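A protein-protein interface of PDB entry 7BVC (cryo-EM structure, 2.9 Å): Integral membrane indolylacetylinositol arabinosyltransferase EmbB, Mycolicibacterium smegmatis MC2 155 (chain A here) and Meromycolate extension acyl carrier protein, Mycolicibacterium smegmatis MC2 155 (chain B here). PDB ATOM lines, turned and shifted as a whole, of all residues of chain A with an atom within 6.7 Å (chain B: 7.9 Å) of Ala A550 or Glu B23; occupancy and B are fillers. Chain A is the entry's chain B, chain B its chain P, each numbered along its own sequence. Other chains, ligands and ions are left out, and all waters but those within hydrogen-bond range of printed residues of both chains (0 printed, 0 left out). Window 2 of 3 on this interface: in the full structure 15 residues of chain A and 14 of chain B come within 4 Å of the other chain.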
ATOM      1  N   PRO A 361      19.408 -30.071  16.217  1.00  0.00           N
ATOM      2  CA  PRO A 361      20.440 -30.540  17.148  1.00  0.00           C
ATOM      3  C   PRO A 361      19.941 -31.497  18.218  1.00  0.00           C
ATOM      4  O   PRO A 361      20.722 -31.870  19.097  1.00  0.00           O
ATOM      5  CB  PRO A 361      20.937 -29.232  17.780  1.00  0.00           C
ATOM      6  CG  PRO A 361      19.764 -28.337  17.739  1.00  0.00           C
ATOM      7  CD  PRO A 361      19.007 -28.680  16.488  1.00  0.00           C
ATOM      8  N   ALA A 362      18.673 -31.902  18.175  1.00  0.00           N
ATOM      9  CA  ALA A 362      18.155 -32.904  19.094  1.00  0.00           C
ATOM     10  C   ALA A 362      18.045 -34.281  18.461  1.00  0.00           C
ATOM     11  O   ALA A 362      18.033 -35.279  19.189  1.00  0.00           O
ATOM     12  CB  ALA A 362      16.779 -32.486  19.624  1.00  0.00           C
ATOM     13  N   LYS A 547       3.990 -26.881  18.565  1.00  0.00           N
ATOM     14  CA  LYS A 547       4.633 -26.054  17.557  1.00  0.00           C
ATOM     15  C   LYS A 547       6.046 -25.635  17.934  1.00  0.00           C
ATOM     16  O   LYS A 547       6.737 -25.035  17.104  1.00  0.00           O
ATOM     17  CB  LYS A 547       3.783 -24.808  17.272  1.00  0.00           C
ATOM     18  CG  LYS A 547       2.427 -25.124  16.665  1.00  0.00           C
ATOM     19  CD  LYS A 547       1.415 -24.028  16.946  1.00  0.00           C
ATOM     20  CE  LYS A 547       0.046 -24.386  16.388  1.00  0.00           C
ATOM     21  NZ  LYS A 547      -0.696 -25.333  17.265  1.00  0.00           N
ATOM     22  N   HIS A 548       6.494 -25.932  19.151  1.00  0.00           N
ATOM     23  CA  HIS A 548       7.869 -25.673  19.572  1.00  0.00           C
ATOM     24  C   HIS A 548       8.342 -26.886  20.360  1.00  0.00           C
ATOM     25  O   HIS A 548       7.830 -27.152  21.452  1.00  0.00           O
ATOM     26  CB  HIS A 548       7.970 -24.403  20.416  1.00  0.00           C
ATOM     27  CG  HIS A 548       7.137 -23.270  19.909  1.00  0.00           C
ATOM     28  ND1 HIS A 548       7.242 -22.785  18.624  1.00  0.00           N
ATOM     29  CD2 HIS A 548       6.187 -22.520  20.517  1.00  0.00           C
ATOM     30  CE1 HIS A 548       6.391 -21.788  18.460  1.00  0.00           C
ATOM     31  NE2 HIS A 548       5.739 -21.607  19.593  1.00  0.00           N
ATOM     32  N   ILE A 549       9.311 -27.616  19.813  1.00  0.00           N
ATOM     33  CA  ILE A 549       9.837 -28.809  20.462  1.00  0.00           C
ATOM     34  C   ILE A 549      11.312 -28.626  20.829  1.00  0.00           C
ATOM     35  O   ILE A 549      11.984 -29.570  21.232  1.00  0.00           O
ATOM     36  CB  ILE A 549       9.595 -30.052  19.584  1.00  0.00           C
ATOM     37  CG1 ILE A 549       8.143 -30.063  19.112  1.00  0.00           C
ATOM     38  CG2 ILE A 549       9.809 -31.336  20.363  1.00  0.00           C
ATOM     39  CD1 ILE A 549       7.819 -31.177  18.155  1.00  0.00           C
ATOM     40  N   ALA A 550      11.821 -27.405  20.680  1.00  0.00           N
ATOM     41  CA  ALA A 550      13.069 -26.961  21.294  1.00  0.00           C
ATOM     42  C   ALA A 550      14.321 -27.624  20.731  1.00  0.00           C
ATOM     43  O   ALA A 550      15.436 -27.242  21.095  1.00  0.00           O
ATOM     44  CB  ALA A 550      13.015 -27.179  22.808  1.00  0.00           C
ATOM     45  N   GLY A 551      14.165 -28.612  19.856  1.00  0.00           N
ATOM     46  CA  GLY A 551      15.331 -29.206  19.234  1.00  0.00           C
ATOM     47  C   GLY A 551      15.134 -29.623  17.793  1.00  0.00           C
ATOM     48  O   GLY A 551      16.055 -30.148  17.165  1.00  0.00           O
ATOM     49  N   VAL A 552      13.941 -29.392  17.254  1.00  0.00           N
ATOM     50  CA  VAL A 552      13.559 -29.886  15.938  1.00  0.00           C
ATOM     51  C   VAL A 552      13.257 -28.700  15.037  1.00  0.00           C
ATOM     52  O   VAL A 552      12.508 -27.795  15.423  1.00  0.00           O
ATOM     53  CB  VAL A 552      12.349 -30.832  16.026  1.00  0.00           C
ATOM     54  CG1 VAL A 552      11.991 -31.366  14.653  1.00  0.00           C
ATOM     55  CG2 VAL A 552      12.641 -31.972  16.985  1.00  0.00           C
ATOM     56  N   ALA B  13      18.442 -14.462  17.450  1.00  0.00           N
ATOM     57  CA  ALA B  13      17.771 -15.627  18.011  1.00  0.00           C
ATOM     58  C   ALA B  13      16.589 -16.067  17.161  1.00  0.00           C
ATOM     59  O   ALA B  13      16.335 -17.268  17.037  1.00  0.00           O
ATOM     60  CB  ALA B  13      17.313 -15.333  19.438  1.00  0.00           C
ATOM     61  N   GLU B  14      15.862 -15.123  16.563  1.00  0.00           N
ATOM     62  CA  GLU B  14      14.728 -15.489  15.724  1.00  0.00           C
ATOM     63  C   GLU B  14      15.154 -16.124  14.408  1.00  0.00           C
ATOM     64  O   GLU B  14      14.319 -16.746  13.744  1.00  0.00           O
ATOM     65  CB  GLU B  14      13.852 -14.268  15.450  1.00  0.00           C
ATOM     66  CG  GLU B  14      14.363 -13.378  14.334  1.00  0.00           C
ATOM     67  CD  GLU B  14      13.384 -12.279  13.977  1.00  0.00           C
ATOM     68  OE1 GLU B  14      12.554 -11.920  14.838  1.00  0.00           O
ATOM     69  OE2 GLU B  14      13.444 -11.775  12.836  1.00  0.00           O
ATOM     70  N   ILE B  16      18.198 -18.099  14.396  1.00  0.00           N
ATOM     71  CA  ILE B  16      18.697 -19.375  14.900  1.00  0.00           C
ATOM     72  C   ILE B  16      17.543 -20.328  15.189  1.00  0.00           C
ATOM     73  O   ILE B  16      17.654 -21.540  14.963  1.00  0.00           O
ATOM     74  CB  ILE B  16      19.574 -19.143  16.147  1.00  0.00           C
ATOM     75  CG1 ILE B  16      20.862 -18.420  15.759  1.00  0.00           C
ATOM     76  CG2 ILE B  16      19.899 -20.457  16.832  1.00  0.00           C
ATOM     77  CD1 ILE B  16      21.859 -18.301  16.889  1.00  0.00           C
ATOM     78  N   GLU B  17      16.415 -19.803  15.668  1.00  0.00           N
ATOM     79  CA  GLU B  17      15.263 -20.643  15.971  1.00  0.00           C
ATOM     80  C   GLU B  17      14.550 -21.110  14.711  1.00  0.00           C
ATOM     81  O   GLU B  17      13.922 -22.176  14.719  1.00  0.00           O
ATOM     82  CB  GLU B  17      14.299 -19.881  16.886  1.00  0.00           C
ATOM     83  CG  GLU B  17      13.192 -20.722  17.499  1.00  0.00           C
ATOM     84  CD  GLU B  17      11.977 -20.827  16.605  1.00  0.00           C
ATOM     85  OE1 GLU B  17      11.734 -19.888  15.819  1.00  0.00           O
ATOM     86  OE2 GLU B  17      11.261 -21.847  16.689  1.00  0.00           O
ATOM     87  N   THR B  20      17.660 -23.802  12.968  1.00  0.00           N
ATOM     88  CA  THR B  20      17.906 -25.024  13.726  1.00  0.00           C
ATOM     89  C   THR B  20      16.702 -25.446  14.560  1.00  0.00           C
ATOM     90  O   THR B  20      16.289 -26.608  14.515  1.00  0.00           O
ATOM     91  CB  THR B  20      19.126 -24.844  14.632  1.00  0.00           C
ATOM     92  OG1 THR B  20      18.881 -23.783  15.561  1.00  0.00           O
ATOM     93  CG2 THR B  20      20.355 -24.509  13.809  1.00  0.00           C
ATOM     94  N   GLY B  21      16.130 -24.520  15.323  1.00  0.00           N
ATOM     95  CA  GLY B  21      15.065 -24.834  16.250  1.00  0.00           C
ATOM     96  C   GLY B  21      15.404 -24.608  17.706  1.00  0.00           C
ATOM     97  O   GLY B  21      14.611 -24.990  18.575  1.00  0.00           O
ATOM     98  N   ILE B  22      16.550 -23.998  18.001  1.00  0.00           N
ATOM     99  CA  ILE B  22      16.955 -23.756  19.379  1.00  0.00           C
ATOM    100  C   ILE B  22      16.110 -22.631  19.961  1.00  0.00           C
ATOM    101  O   ILE B  22      15.933 -21.579  19.334  1.00  0.00           O
ATOM    102  CB  ILE B  22      18.452 -23.422  19.441  1.00  0.00           C
ATOM    103  CG1 ILE B  22      19.282 -24.654  19.079  1.00  0.00           C
ATOM    104  CG2 ILE B  22      18.836 -22.903  20.816  1.00  0.00           C
ATOM    105  CD1 ILE B  22      20.763 -24.391  19.028  1.00  0.00           C
ATOM    106  N   GLU B  23      15.578 -22.854  21.159  1.00  0.00           N
ATOM    107  CA  GLU B  23      14.739 -21.850  21.795  1.00  0.00           C
ATOM    108  C   GLU B  23      15.540 -20.574  22.046  1.00  0.00           C
ATOM    109  O   GLU B  23      16.735 -20.638  22.348  1.00  0.00           O
ATOM    110  CB  GLU B  23      14.174 -22.379  23.112  1.00  0.00           C
ATOM    111  CG  GLU B  23      13.321 -23.624  22.962  1.00  0.00           C
ATOM    112  CD  GLU B  23      12.122 -23.412  22.057  1.00  0.00           C
ATOM    113  OE1 GLU B  23      12.217 -23.728  20.853  1.00  0.00           O
ATOM    114  OE2 GLU B  23      11.082 -22.929  22.551  1.00  0.00           O
ATOM    115  N   PRO B  24      14.912 -19.402  21.929  1.00  0.00           N
ATOM    116  CA  PRO B  24      15.661 -18.145  22.076  1.00  0.00           C
ATOM    117  C   PRO B  24      16.035 -17.832  23.516  1.00  0.00           C
ATOM    118  O   PRO B  24      16.622 -16.781  23.793  1.00  0.00           O
ATOM    119  CB  PRO B  24      14.696 -17.099  21.510  1.00  0.00           C
ATOM    120  CG  PRO B  24      13.349 -17.687  21.728  1.00  0.00           C
ATOM    121  CD  PRO B  24      13.507 -19.170  21.560  1.00  0.00           C
ATOM    122  N   SER B  25      15.707 -18.729  24.442  1.00  0.00           N
ATOM    123  CA  SER B  25      16.116 -18.584  25.830  1.00  0.00           C
ATOM    124  C   SER B  25      17.502 -19.155  26.093  1.00  0.00           C
ATOM    125  O   SER B  25      17.998 -19.051  27.219  1.00  0.00           O
ATOM    126  CB  SER B  25      15.097 -19.257  26.755  1.00  0.00           C
ATOM    127  OG  SER B  25      15.083 -20.661  26.563  1.00  0.00           O
ATOM    128  N   GLU B  26      18.133 -19.751  25.082  1.00  0.00           N
ATOM    129  CA  GLU B  26      19.483 -20.282  25.205  1.00  0.00           C
ATOM    130  C   GLU B  26      20.543 -19.361  24.622  1.00  0.00           C
ATOM    131  O   GLU B  26      21.722 -19.500  24.969  1.00  0.00           O
ATOM    132  CB  GLU B  26      19.582 -21.647  24.514  1.00  0.00           C
ATOM    133  CG  GLU B  26      18.408 -22.567  24.784  1.00  0.00           C
ATOM    134  CD  GLU B  26      18.507 -23.250  26.130  1.00  0.00           C
ATOM    135  OE1 GLU B  26      19.610 -23.254  26.714  1.00  0.00           O
ATOM    136  OE2 GLU B  26      17.482 -23.783  26.605  1.00  0.00           O
ATOM    137  N   VAL B  27      20.157 -18.428  23.753  1.00  0.00           N
ATOM    138  CA  VAL B  27      21.104 -17.563  23.055  1.00  0.00           C
ATOM    139  C   VAL B  27      21.537 -16.471  24.029  1.00  0.00           C
ATOM    140  O   VAL B  27      20.849 -15.464  24.201  1.00  0.00           O
ATOM    141  CB  VAL B  27      20.503 -16.977  21.775  1.00  0.00           C
ATOM    142  CG1 VAL B  27      21.512 -16.084  21.075  1.00  0.00           C
ATOM    143  CG2 VAL B  27      20.044 -18.093  20.851  1.00  0.00           C
ATOM    144  N   THR B  28      22.681 -16.671  24.668  1.00  0.00           N
ATOM    145  CA  THR B  28      23.291 -15.716  25.577  1.00  0.00           C
ATOM    146  C   THR B  28      24.651 -15.296  25.030  1.00  0.00           C
ATOM    147  O   THR B  28      25.259 -16.020  24.234  1.00  0.00           O
ATOM    148  CB  THR B  28      23.448 -16.319  26.981  1.00  0.00           C
ATOM    149  OG1 THR B  28      24.534 -17.253  26.985  1.00  0.00           O
ATOM    150  CG2 THR B  28      22.172 -17.028  27.406  1.00  0.00           C
ATOM    151  N   LYS B  31      27.739 -18.004  24.763  1.00  0.00           N
ATOM    152  CA  LYS B  31      27.552 -19.341  24.216  1.00  0.00           C
ATOM    153  C   LYS B  31      28.339 -19.489  22.922  1.00  0.00           C
ATOM    154  O   LYS B  31      28.219 -18.654  22.020  1.00  0.00           O
ATOM    155  CB  LYS B  31      26.071 -19.618  23.961  1.00  0.00           C
ATOM    156  CG  LYS B  31      25.255 -19.808  25.222  1.00  0.00           C
ATOM    157  CD  LYS B  31      25.439 -21.197  25.799  1.00  0.00           C
ATOM    158  CE  LYS B  31      24.485 -21.443  26.954  1.00  0.00           C
ATOM    159  NZ  LYS B  31      23.072 -21.227  26.542  1.00  0.00           N
ATOM    160  N   LEU B  37      25.920 -24.559  21.967  1.00  0.00           N
ATOM    161  CA  LEU B  37      24.878 -24.717  20.958  1.00  0.00           C
ATOM    162  C   LEU B  37      25.466 -25.507  19.797  1.00  0.00           C
ATOM    163  O   LEU B  37      26.324 -24.999  19.070  1.00  0.00           O
ATOM    164  CB  LEU B  37      24.363 -23.359  20.487  1.00  0.00           C
ATOM    165  CG  LEU B  37      24.099 -22.301  21.554  1.00  0.00           C
ATOM    166  CD1 LEU B  37      23.901 -20.939  20.914  1.00  0.00           C
ATOM    167  CD2 LEU B  37      22.889 -22.687  22.384  1.00  0.00           C
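Ala A550 touches just these residues of chain B: Gly B21 and Glu B23. Printed residues of chain B within 4 Å of Gly A551: Gly B21. Of the printed residues of chain A, Thr B20 touches Pro A361 and Val A552. Of the printed residues of chain A, Gly B21 touches Ala A550 (3.4 Å), Gly A551 (3.9 Å) and Val A552 (3.999 Å). Of chain A, only Ala A550 (3.4 Å) comes within 4 Å of Glu B23.
The backbone NH (N) of Gly B21 lies within hydrogen-bond range of the backbone carbonyl oxygen (O) of Ile B16 (3.4 Å). O of Ile B16 lies within hydrogen-bond range of OG1 of Thr B20 (2.6 Å). The side-chain hydroxyl of Thr B20 sits at hydrogen-bond distance from the backbone NH of Ile B22 (3.4 Å). N of Ala A362 lies within hydrogen-bond range of O of Gly A551 (3.3 Å).
Hydrophobic or aromatic side chains of chain A within 4 Å of the printed part of chain B: Pro A361 and Ala A550. Among the printed residues, no Asp or Glu carboxylate lies within 4 Å of a Lys or Arg side-chain nitrogen of the other chain.
The backbone carbonyl oxygen of Ala A550 lies close to the backbone carbonyl oxygen of Gly B21 (3.5 Å).
Thr B20 touches Pro A361 (O to CD, 3.9 Å). Ile B22 touches Pro A361 (CG1 to CG, 3.9 Å). Glu B23 touches Ala A550. Gly B21 touches Gly A551 (O to N, 3.9 Å). O of Thr B20 touches C of Val A552 (3.7 Å). Val A552 touches Gly B21 (O to CA, 3.999 Å).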
